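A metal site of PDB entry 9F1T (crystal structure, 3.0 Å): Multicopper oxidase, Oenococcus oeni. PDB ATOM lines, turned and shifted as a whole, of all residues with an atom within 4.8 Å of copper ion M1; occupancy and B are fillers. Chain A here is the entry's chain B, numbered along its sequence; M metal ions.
A ring nitrogen (NE2) of His 397 binds copper ion M1 (1.9 Å). NE2 of His 149 is bound to copper ion M1, at 2.2 Å. Copper ion M1 is bound by a ring nitrogen (NE2) of His 445. Copper ion M1 has three donor atoms within binding distance.
O of His 445 sits at hydrogen-bond distance from N of His 395, at 2.9 Å. O of Met 443 lies within hydrogen-bond range of N of His 397, 2.9 Å away.
Merely in contact with copper ion M1: His 106 (3.6 Å) and His 395 (3.9 Å). Within 4 Å of copper ion M1: His 106, His 149, His 395, His 397 and His 445. Along chain A the residues within 4 Å of copper ion M1 span positions 106 to 445. The nearest printed residue that does not touch copper ion M1 is Met 457 (4.04 Å).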
ATOM      1  N   HIS A 106     -27.216  22.346  19.053  1.00  0.00           N
ATOM      2  CA  HIS A 106     -25.890  22.917  18.980  1.00  0.00           C
ATOM      3  C   HIS A 106     -25.105  22.220  17.876  1.00  0.00           C
ATOM      4  O   HIS A 106     -24.977  21.001  17.894  1.00  0.00           O
ATOM      5  CB  HIS A 106     -25.135  22.826  20.311  1.00  0.00           C
ATOM      6  CG  HIS A 106     -23.739  23.346  20.173  1.00  0.00           C
ATOM      7  ND1 HIS A 106     -23.439  24.373  19.314  1.00  0.00           N
ATOM      8  CD2 HIS A 106     -22.586  22.990  20.747  1.00  0.00           C
ATOM      9  CE1 HIS A 106     -22.145  24.623  19.369  1.00  0.00           C
ATOM     10  NE2 HIS A 106     -21.608  23.796  20.238  1.00  0.00           N
ATOM     11  N   HIS A 149     -27.942  21.176  23.610  1.00  0.00           N
ATOM     12  CA  HIS A 149     -27.233  21.989  24.580  1.00  0.00           C
ATOM     13  C   HIS A 149     -28.165  22.796  25.489  1.00  0.00           C
ATOM     14  O   HIS A 149     -27.896  23.966  25.734  1.00  0.00           O
ATOM     15  CB  HIS A 149     -26.358  23.003  23.850  1.00  0.00           C
ATOM     16  CG  HIS A 149     -25.069  23.326  24.524  1.00  0.00           C
ATOM     17  ND1 HIS A 149     -24.978  23.574  25.877  1.00  0.00           N
ATOM     18  CD2 HIS A 149     -23.821  23.486  24.034  1.00  0.00           C
ATOM     19  CE1 HIS A 149     -23.716  23.847  26.186  1.00  0.00           C
ATOM     20  NE2 HIS A 149     -23.006  23.802  25.081  1.00  0.00           N
ATOM     21  N   HIS A 395     -13.799  23.817  25.126  1.00  0.00           N
ATOM     22  CA  HIS A 395     -14.447  24.005  23.844  1.00  0.00           C
ATOM     23  C   HIS A 395     -14.889  25.465  23.710  1.00  0.00           C
ATOM     24  O   HIS A 395     -15.349  26.046  24.694  1.00  0.00           O
ATOM     25  CB  HIS A 395     -15.663  23.074  23.731  1.00  0.00           C
ATOM     26  CG  HIS A 395     -16.458  23.283  22.475  1.00  0.00           C
ATOM     27  ND1 HIS A 395     -15.867  23.455  21.246  1.00  0.00           N
ATOM     28  CD2 HIS A 395     -17.774  23.353  22.269  1.00  0.00           C
ATOM     29  CE1 HIS A 395     -16.814  23.635  20.332  1.00  0.00           C
ATOM     30  NE2 HIS A 395     -17.968  23.571  20.933  1.00  0.00           N
ATOM     31  N   HIS A 397     -17.403  27.850  21.200  1.00  0.00           N
ATOM     32  CA  HIS A 397     -18.410  27.924  20.157  1.00  0.00           C
ATOM     33  C   HIS A 397     -18.010  28.964  19.114  1.00  0.00           C
ATOM     34  O   HIS A 397     -17.356  29.953  19.429  1.00  0.00           O
ATOM     35  CB  HIS A 397     -19.794  28.309  20.708  1.00  0.00           C
ATOM     36  CG  HIS A 397     -20.451  27.305  21.589  1.00  0.00           C
ATOM     37  ND1 HIS A 397     -21.820  27.278  21.712  1.00  0.00           N
ATOM     38  CD2 HIS A 397     -19.997  26.347  22.410  1.00  0.00           C
ATOM     39  CE1 HIS A 397     -22.172  26.326  22.565  1.00  0.00           C
ATOM     40  NE2 HIS A 397     -21.077  25.747  23.007  1.00  0.00           N
ATOM     41  N   MET A 443     -20.417  30.528  23.526  1.00  0.00           N
ATOM     42  CA  MET A 443     -20.053  29.881  24.769  1.00  0.00           C
ATOM     43  C   MET A 443     -18.611  29.412  24.703  1.00  0.00           C
ATOM     44  O   MET A 443     -18.062  29.194  23.629  1.00  0.00           O
ATOM     45  CB  MET A 443     -20.927  28.664  25.050  1.00  0.00           C
ATOM     46  CG  MET A 443     -22.374  28.804  24.645  1.00  0.00           C
ATOM     47  SD  MET A 443     -23.079  30.226  25.505  1.00  0.00           S
ATOM     48  CE  MET A 443     -23.908  30.997  24.103  1.00  0.00           C
ATOM     49  N   HIS A 445     -16.546  26.499  27.409  1.00  0.00           N
ATOM     50  CA  HIS A 445     -16.826  25.652  28.564  1.00  0.00           C
ATOM     51  C   HIS A 445     -16.053  24.344  28.524  1.00  0.00           C
ATOM     52  O   HIS A 445     -15.494  23.957  27.495  1.00  0.00           O
ATOM     53  CB  HIS A 445     -18.330  25.324  28.632  1.00  0.00           C
ATOM     54  CG  HIS A 445     -18.843  24.528  27.478  1.00  0.00           C
ATOM     55  ND1 HIS A 445     -19.258  23.230  27.632  1.00  0.00           N
ATOM     56  CD2 HIS A 445     -19.019  24.811  26.170  1.00  0.00           C
ATOM     57  CE1 HIS A 445     -19.674  22.745  26.474  1.00  0.00           C
ATOM     58  NE2 HIS A 445     -19.520  23.690  25.565  1.00  0.00           N
ATOM     59  N   MET A 457     -19.192  27.103  32.474  1.00  0.00           N
ATOM     60  CA  MET A 457     -19.453  27.711  31.188  1.00  0.00           C
ATOM     61  C   MET A 457     -19.337  29.220  31.306  1.00  0.00           C
ATOM     62  O   MET A 457     -19.409  29.755  32.416  1.00  0.00           O
ATOM     63  CB  MET A 457     -20.850  27.329  30.716  1.00  0.00           C
ATOM     64  CG  MET A 457     -21.234  27.861  29.359  1.00  0.00           C
ATOM     65  SD  MET A 457     -22.572  26.845  28.701  1.00  0.00           S
ATOM     66  CE  MET A 457     -21.718  26.164  27.287  1.00  0.00           C
HETATM   67 CU    CU M   1     -21.216  24.097  23.852  1.00  0.00          CU
HETATM   68 CU    CU M   2     -19.697  23.934  20.491  1.00  0.00          CU
HETATM   69 CU    CU M   3     -20.126  20.359  21.762  1.00  0.00          CU
